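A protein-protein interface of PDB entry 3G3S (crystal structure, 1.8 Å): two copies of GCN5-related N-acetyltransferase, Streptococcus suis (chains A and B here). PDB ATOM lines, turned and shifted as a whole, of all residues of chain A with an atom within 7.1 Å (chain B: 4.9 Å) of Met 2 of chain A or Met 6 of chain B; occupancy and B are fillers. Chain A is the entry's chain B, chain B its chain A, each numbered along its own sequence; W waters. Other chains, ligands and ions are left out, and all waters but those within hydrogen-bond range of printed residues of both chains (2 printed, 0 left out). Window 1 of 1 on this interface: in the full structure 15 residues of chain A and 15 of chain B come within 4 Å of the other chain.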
ATOM      1  N   GLY A   1      17.129   2.166   8.057  1.00  0.00           N
ATOM      2  CA  GLY A   1      16.766   0.781   7.623  1.00  0.00           C
ATOM      3  C   GLY A   1      16.044   0.742   6.281  1.00  0.00           C
ATOM      4  O   GLY A   1      16.110   1.700   5.497  1.00  0.00           O
ATOM      5  N   MET A   2      15.334  -0.352   6.019  1.00  0.00           N
ATOM      6  CA  MET A   2      14.648  -0.545   4.754  1.00  0.00           C
ATOM      7  C   MET A   2      13.564   0.481   4.495  1.00  0.00           C
ATOM      8  O   MET A   2      13.412   0.955   3.347  1.00  0.00           O
ATOM      9  CB  MET A   2      14.044  -1.935   4.693  1.00  0.00           C
ATOM     10  CG  MET A   2      15.065  -3.039   4.577  1.00  0.00           C
ATOM     11  SD  MET A   2      14.329  -4.797   4.519  1.00  0.00           S
ATOM     12  CE  MET A   2      13.231  -4.492   2.979  1.00  0.00           C
ATOM     13  N   ALA A   3      12.800   0.818   5.535  1.00  0.00           N
ATOM     14  CA  ALA A   3      11.747   1.809   5.416  1.00  0.00           C
ATOM     15  C   ALA A   3      12.312   3.223   5.161  1.00  0.00           C
ATOM     16  O   ALA A   3      11.734   3.999   4.376  1.00  0.00           O
ATOM     17  CB  ALA A   3      10.850   1.795   6.623  1.00  0.00           C
ATOM     18  N   GLU A   4      13.428   3.568   5.798  1.00  0.00           N
ATOM     19  CA  GLU A   4      14.031   4.861   5.547  1.00  0.00           C
ATOM     20  C   GLU A   4      14.503   4.900   4.083  1.00  0.00           C
ATOM     21  O   GLU A   4      14.309   5.888   3.378  1.00  0.00           O
ATOM     22  CB  GLU A   4      15.193   5.150   6.511  1.00  0.00           C
ATOM     23  CG  GLU A   4      15.908   6.506   6.240  1.00  0.00           C
ATOM     24  N   GLN A   5      15.111   3.812   3.632  1.00  0.00           N
ATOM     25  CA  GLN A   5      15.591   3.728   2.250  1.00  0.00           C
ATOM     26  C   GLN A   5      14.483   3.924   1.197  1.00  0.00           C
ATOM     27  O   GLN A   5      14.693   4.540   0.164  1.00  0.00           O
ATOM     28  CB  GLN A   5      16.322   2.403   2.028  1.00  0.00           C
ATOM     29  CG  GLN A   5      17.626   2.339   2.776  1.00  0.00           C
ATOM     30  CD  GLN A   5      18.621   3.376   2.283  1.00  0.00           C
ATOM     31  OE1 GLN A   5      18.833   4.408   2.930  1.00  0.00           O
ATOM     32  NE2 GLN A   5      19.185   3.143   1.100  1.00  0.00           N
ATOM     33  N   MET A   6      13.309   3.406   1.474  1.00  0.00           N
ATOM     34  CA  MET A   6      12.214   3.565   0.575  1.00  0.00           C
ATOM     35  C   MET A   6      11.696   5.024   0.614  1.00  0.00           C
ATOM     36  O   MET A   6      11.228   5.555  -0.422  1.00  0.00           O
ATOM     37  CB  MET A   6      11.110   2.545   0.893  1.00  0.00           C
ATOM     38  CG  MET A   6       9.906   2.648  -0.033  1.00  0.00           C
ATOM     39  SD  MET A   6      10.281   2.418  -1.913  1.00  0.00           S
ATOM     40  CE  MET A   6      10.526   0.731  -2.025  1.00  0.00           C
ATOM     41  N   ARG A   7      11.771   5.678   1.770  1.00  0.00           N
ATOM     42  CA  ARG A   7      11.352   7.087   1.859  1.00  0.00           C
ATOM     43  C   ARG A   7      12.211   7.996   0.969  1.00  0.00           C
ATOM     44  O   ARG A   7      11.707   8.934   0.344  1.00  0.00           O
ATOM     45  CB  ARG A   7      11.344   7.590   3.307  1.00  0.00           C
ATOM     46  CG  ARG A   7      10.224   6.966   4.128  1.00  0.00           C
ATOM     47  CD  ARG A   7      10.060   7.619   5.482  1.00  0.00           C
ATOM     48  NE  ARG A   7      11.084   7.215   6.434  1.00  0.00           N
ATOM     49  CZ  ARG A   7      10.961   6.254   7.343  1.00  0.00           C
ATOM     50  NH1 ARG A   7       9.855   5.541   7.443  1.00  0.00           N
ATOM     51  NH2 ARG A   7      11.969   6.010   8.166  1.00  0.00           N
ATOM     52  N   GLY A  27       3.574  -0.303  -1.791  1.00  0.00           N
ATOM     53  CA  GLY A  27       4.091  -1.586  -1.308  1.00  0.00           C
ATOM     54  C   GLY A  27       3.377  -2.888  -1.530  1.00  0.00           C
ATOM     55  O   GLY A  27       3.984  -3.944  -1.425  1.00  0.00           O
ATOM     56  N   ASP A  31       6.675  -3.061  -8.101  1.00  0.00           N
ATOM     57  CA  ASP A  31       7.972  -3.167  -7.464  1.00  0.00           C
ATOM     58  C   ASP A  31       8.779  -1.904  -7.743  1.00  0.00           C
ATOM     59  O   ASP A  31       8.372  -1.015  -8.497  1.00  0.00           O
ATOM     60  CB  ASP A  31       8.681  -4.456  -7.926  1.00  0.00           C
ATOM     61  CG  ASP A  31       9.692  -5.007  -6.897  1.00  0.00           C
ATOM     62  OD1 ASP A  31      10.116  -4.294  -5.964  1.00  0.00           O
ATOM     63  OD2 ASP A  31      10.089  -6.173  -7.032  1.00  0.00           O
ATOM     64  N   MET B   2      12.991  -3.785  -4.269  1.00  0.00           N
ATOM     65  CA  MET B   2      12.845  -3.285  -2.917  1.00  0.00           C
ATOM     66  C   MET B   2      11.457  -3.529  -2.324  1.00  0.00           C
ATOM     67  O   MET B   2      11.359  -3.881  -1.157  1.00  0.00           O
ATOM     68  CB  MET B   2      13.183  -1.792  -2.821  1.00  0.00           C
ATOM     69  CG  MET B   2      14.700  -1.514  -2.848  1.00  0.00           C
ATOM     70  SD  MET B   2      15.037   0.366  -2.870  1.00  0.00           S
ATOM     71  CE  MET B   2      14.622   1.067  -1.234  1.00  0.00           C
ATOM     72  N   ALA B   3      10.400  -3.328  -3.112  1.00  0.00           N
ATOM     73  CA  ALA B   3       9.041  -3.534  -2.623  1.00  0.00           C
ATOM     74  C   ALA B   3       8.745  -5.018  -2.446  1.00  0.00           C
ATOM     75  O   ALA B   3       7.980  -5.377  -1.586  1.00  0.00           O
ATOM     76  CB  ALA B   3       8.037  -2.915  -3.555  1.00  0.00           C
ATOM     77  N   GLU B   4       9.327  -5.878  -3.266  1.00  0.00           N
ATOM     78  CA  GLU B   4       9.124  -7.308  -3.098  1.00  0.00           C
ATOM     79  C   GLU B   4       9.799  -7.744  -1.805  1.00  0.00           C
ATOM     80  O   GLU B   4       9.228  -8.506  -1.022  1.00  0.00           O
ATOM     81  CB  GLU B   4       9.660  -8.099  -4.313  1.00  0.00           C
ATOM     82  CG  GLU B   4       9.657  -9.612  -4.165  1.00  0.00           C
ATOM     83  CD  GLU B   4       8.266 -10.176  -3.934  1.00  0.00           C
ATOM     84  OE1 GLU B   4       7.321  -9.739  -4.637  1.00  0.00           O
ATOM     85  OE2 GLU B   4       8.125 -11.071  -3.058  1.00  0.00           O
ATOM     86  N   GLN B   5      11.018  -7.255  -1.572  1.00  0.00           N
ATOM     87  CA  GLN B   5      11.720  -7.620  -0.344  1.00  0.00           C
ATOM     88  C   GLN B   5      10.952  -7.120   0.882  1.00  0.00           C
ATOM     89  O   GLN B   5      10.860  -7.842   1.888  1.00  0.00           O
ATOM     90  CB  GLN B   5      13.177  -7.134  -0.347  1.00  0.00           C
ATOM     91  CG  GLN B   5      13.997  -7.785  -1.455  1.00  0.00           C
ATOM     92  CD  GLN B   5      13.993  -9.318  -1.391  1.00  0.00           C
ATOM     93  OE1 GLN B   5      13.352  -9.986  -2.215  1.00  0.00           O
ATOM     94  NE2 GLN B   5      14.697  -9.877  -0.405  1.00  0.00           N
ATOM     95  N   MET B   6      10.361  -5.930   0.792  1.00  0.00           N
ATOM     96  CA  MET B   6       9.598  -5.444   1.917  1.00  0.00           C
ATOM     97  C   MET B   6       8.359  -6.337   2.156  1.00  0.00           C
ATOM     98  O   MET B   6       8.019  -6.586   3.311  1.00  0.00           O
ATOM     99  CB  MET B   6       9.230  -3.989   1.777  1.00  0.00           C
ATOM    100  CG  MET B   6       8.490  -3.416   3.016  1.00  0.00           C
ATOM    101  SD  MET B   6       9.286  -3.691   4.791  1.00  0.00           S
ATOM    102  CE  MET B   6      10.551  -2.392   4.656  1.00  0.00           C
ATOM    103  N   ARG B   7       7.742  -6.864   1.102  1.00  0.00           N
ATOM    104  CA  ARG B   7       6.602  -7.785   1.255  1.00  0.00           C
ATOM    105  C   ARG B   7       7.009  -9.076   1.955  1.00  0.00           C
ATOM    106  O   ARG B   7       6.268  -9.613   2.772  1.00  0.00           O
ATOM    107  CB  ARG B   7       5.916  -8.094  -0.090  1.00  0.00           C
ATOM    108  CG  ARG B   7       5.168  -6.943  -0.641  1.00  0.00           C
ATOM    109  CD  ARG B   7       4.312  -7.304  -1.866  1.00  0.00           C
ATOM    110  NE  ARG B   7       5.057  -7.491  -3.127  1.00  0.00           N
ATOM    111  CZ  ARG B   7       5.442  -6.505  -3.939  1.00  0.00           C
ATOM    112  NH1 ARG B   7       5.230  -5.233  -3.624  1.00  0.00           N
ATOM    113  NH2 ARG B   7       6.082  -6.789  -5.063  1.00  0.00           N
ATOM    114  N   ARG B   8       8.196  -9.573   1.636  1.00  0.00           N
ATOM    115  CA  ARG B   8       8.719 -10.760   2.280  1.00  0.00           C
ATOM    116  C   ARG B   8       8.946 -10.515   3.787  1.00  0.00           C
ATOM    117  O   ARG B   8       8.578 -11.335   4.639  1.00  0.00           O
ATOM    118  CB  ARG B   8      10.033 -11.183   1.610  1.00  0.00           C
ATOM    119  CG  ARG B   8       9.884 -11.625   0.154  1.00  0.00           C
ATOM    120  N   VAL B   9       9.532  -9.365   4.105  1.00  0.00           N
ATOM    121  CA  VAL B   9       9.795  -8.970   5.474  1.00  0.00           C
ATOM    122  C   VAL B   9       8.487  -8.835   6.231  1.00  0.00           C
ATOM    123  O   VAL B   9       8.364  -9.287   7.370  1.00  0.00           O
ATOM    124  CB  VAL B   9      10.578  -7.645   5.555  1.00  0.00           C
ATOM    125  CG1 VAL B   9      10.813  -7.281   6.989  1.00  0.00           C
ATOM    126  CG2 VAL B   9      11.907  -7.788   4.850  1.00  0.00           C
ATOM    127  N   ALA B  10       7.484  -8.269   5.587  1.00  0.00           N
ATOM    128  CA  ALA B  10       6.217  -8.100   6.270  1.00  0.00           C
ATOM    129  C   ALA B  10       5.643  -9.458   6.654  1.00  0.00           C
ATOM    130  O   ALA B  10       5.011  -9.577   7.708  1.00  0.00           O
ATOM    131  CB  ALA B  10       5.264  -7.356   5.394  1.00  0.00           C
ATOM    132  N   LEU B  25       5.769  -1.025   9.090  1.00  0.00           N
ATOM    133  CA  LEU B  25       5.584  -1.653   7.771  1.00  0.00           C
ATOM    134  C   LEU B  25       4.875  -0.788   6.699  1.00  0.00           C
ATOM    135  O   LEU B  25       5.104  -1.029   5.528  1.00  0.00           O
ATOM    136  CB  LEU B  25       4.839  -2.963   7.946  1.00  0.00           C
ATOM    137  CG  LEU B  25       5.491  -4.114   8.704  1.00  0.00           C
ATOM    138  CD1 LEU B  25       4.523  -5.241   8.896  1.00  0.00           C
ATOM    139  CD2 LEU B  25       6.824  -4.633   7.996  1.00  0.00           C
ATOM    140  N   ASP B  31      10.943   2.246  11.240  1.00  0.00           N
ATOM    141  CA  ASP B  31      11.864   1.656  10.289  1.00  0.00           C
ATOM    142  C   ASP B  31      11.886   0.164  10.478  1.00  0.00           C
ATOM    143  O   ASP B  31      11.403  -0.396  11.461  1.00  0.00           O
ATOM    144  CB  ASP B  31      13.238   2.268  10.491  1.00  0.00           C
ATOM    145  CG  ASP B  31      14.112   2.262   9.219  1.00  0.00           C
ATOM    146  OD1 ASP B  31      13.859   1.527   8.227  1.00  0.00           O
ATOM    147  OD2 ASP B  31      15.062   3.050   9.217  1.00  0.00           O
ATOM    148  N   ILE B  32      12.493  -0.486   9.512  1.00  0.00           N
ATOM    149  CA  ILE B  32      12.569  -1.921   9.445  1.00  0.00           C
ATOM    150  C   ILE B  32      14.000  -2.368   9.152  1.00  0.00           C
ATOM    151  O   ILE B  32      14.587  -1.881   8.232  1.00  0.00           O
ATOM    152  CB  ILE B  32      11.720  -2.421   8.318  1.00  0.00           C
ATOM    153  CG1 ILE B  32      10.215  -2.134   8.643  1.00  0.00           C
ATOM    154  CG2 ILE B  32      11.906  -3.920   8.145  1.00  0.00           C
ATOM    155  CD1 ILE B  32       9.648  -2.927   9.798  1.00  0.00           C
ATOM    156  N   VAL B  34      16.583  -6.024   8.937  1.00  0.00           N
ATOM    157  CA  VAL B  34      16.508  -7.449   8.742  1.00  0.00           C
ATOM    158  C   VAL B  34      17.905  -8.019   8.792  1.00  0.00           C
ATOM    159  O   VAL B  34      18.891  -7.275   8.766  1.00  0.00           O
ATOM    160  CB  VAL B  34      15.794  -7.835   7.410  1.00  0.00           C
ATOM    161  CG1 VAL B  34      14.311  -7.416   7.441  1.00  0.00           C
ATOM    162  CG2 VAL B  34      16.510  -7.228   6.181  1.00  0.00           C
HETATM  163  O   HOH W   1       6.465  -3.664  -0.327  1.00  0.00           O
HETATM  164  O   HOH W   2       4.670  -2.139  -4.122  1.00  0.00           O
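N of Met 2 of chain B sits at hydrogen-bond distance from OD1 of Asp 31 of chain A (3.4 Å). N of Ala 3 of chain B lies within hydrogen-bond range of OD1 of Asp 31 of chain A, at 3.0 Å. The side-chain carboxylate (OD1) of Asp 31 of chain A sits at hydrogen-bond distance from the backbone NH (N) of Glu 4 of chain B, 3.2 Å away. O of Gly 27 of chain A sits at hydrogen-bond distance from NH1 of Arg 7 of chain B, 2.8 Å away. OD2 of Asp 31 of chain B lies within hydrogen-bond range of N of Gly 1 of chain A, 2.5 Å away. OD1 of Asp 31 of chain B lies within hydrogen-bond range of N of Met 2 of chain A. OD1 of Asp 31 of chain B lies within hydrogen-bond range of N of Ala 3 of chain A, at 3.0 Å. OD1 of Asp 31 of chain B sits at hydrogen-bond distance from N of Glu 4 of chain A. The backbone carbonyl oxygen of Ile 32 of chain B lies within hydrogen-bond range of the backbone NH of Met 2 of chain A (2.8 Å).
Water W1 bridges the backbone carbonyl oxygen (O) of Ala 3 of chain B (2.6 Å) and the backbone carbonyl oxygen (O) of Gly 27 of chain A (2.7 Å). Water W2 lies within hydrogen-bond range of the backbone NH of Gly 27 of chain A (3.2 Å) and the guanidinium group of Arg 7 of chain B (3.2 Å).
Of the 9 printed residues of chain A, 8 touch a printed residue of chain B. Printed residues of chain A that touch a printed residue of chain B: Gly 1, Met 2, Ala 3, Glu 4, Gln 5, Met 6, Gly 27 and Asp 31. Hydrophobic or aromatic side chains of chain A within 4 Å of the printed part of chain B: Met 2, Ala 3 and Met 6. Of the 13 printed residues of chain B, 9 touch a printed residue of chain A. Hydrophobic or aromatic side chains of chain B that line the printed part of chain A: Met 2, Ala 3, Met 6, Val 9 and Val 34. Among the printed residues, 15 pairs touch across the chains.
Among the printed residues, merely in contact across the chains: Gly 1 of chain A with Ile 32 of chain B (3.5 Å), Met 2 of chain A with Met 6 of chain B (3.5 Å), Met 2 of chain A with Val 9 of chain B (3.9 Å), Met 2 of chain A with Val 34 of chain B (3.7 Å), Gln 5 of chain A with Met 2 of chain B (3.7 Å) and Met 6 of chain A with Met 2 of chain B (3.7 Å).
The guanidinium group (NH1) of Arg 7 of chain B lies close to the backbone carbonyl oxygen (O) of Ala 3 of chain B, 3.4 Å away. OE1 of Glu 4 of chain B lies within salt-bridge range of NH2 of Arg 7 of chain B, 3.2 Å away.
Met 2 of chain A touches Met 6 of chain B, and with the chains exchanged Met 6 of chain A touches Met 2 of chain B. Ala 3 of chain A touches Asp 31 of chain B, and with the chains exchanged Asp 31 of chain A touches Ala 3 of chain B. Glu 4 of chain A touches Asp 31 of chain B, and with the chains exchanged Asp 31 of chain A touches Glu 4 of chain B. Gln 5 of chain A touches Met 2 of chain B, but with the chains exchanged Met 2 of chain A does not touch Gln 5 of chain B (4.1 Å). Positions printed for both chains: 2, 3, 4, 5, 6, 7 and 31.
Of chain B, only Met 6 (3.5 Å), Val 9 (3.9 Å), Asp 31 (3.3 Å), Ile 32 (2.8 Å) and Val 34 (3.7 Å) come within 4 Å of Met 2 of chain A. Of the printed residues of chain B, Gln 5 of chain A touches Met 2 (3.7 Å). Printed residues of chain B within 4 Å of Met 6 of chain A: Met 2. Arg 7 of chain A touches none of the printed residues of chain B. Of the printed residues of chain B, Gly 27 of chain A touches Arg 7. Of the printed residues of chain A, Val 9 of chain B touches Met 2.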
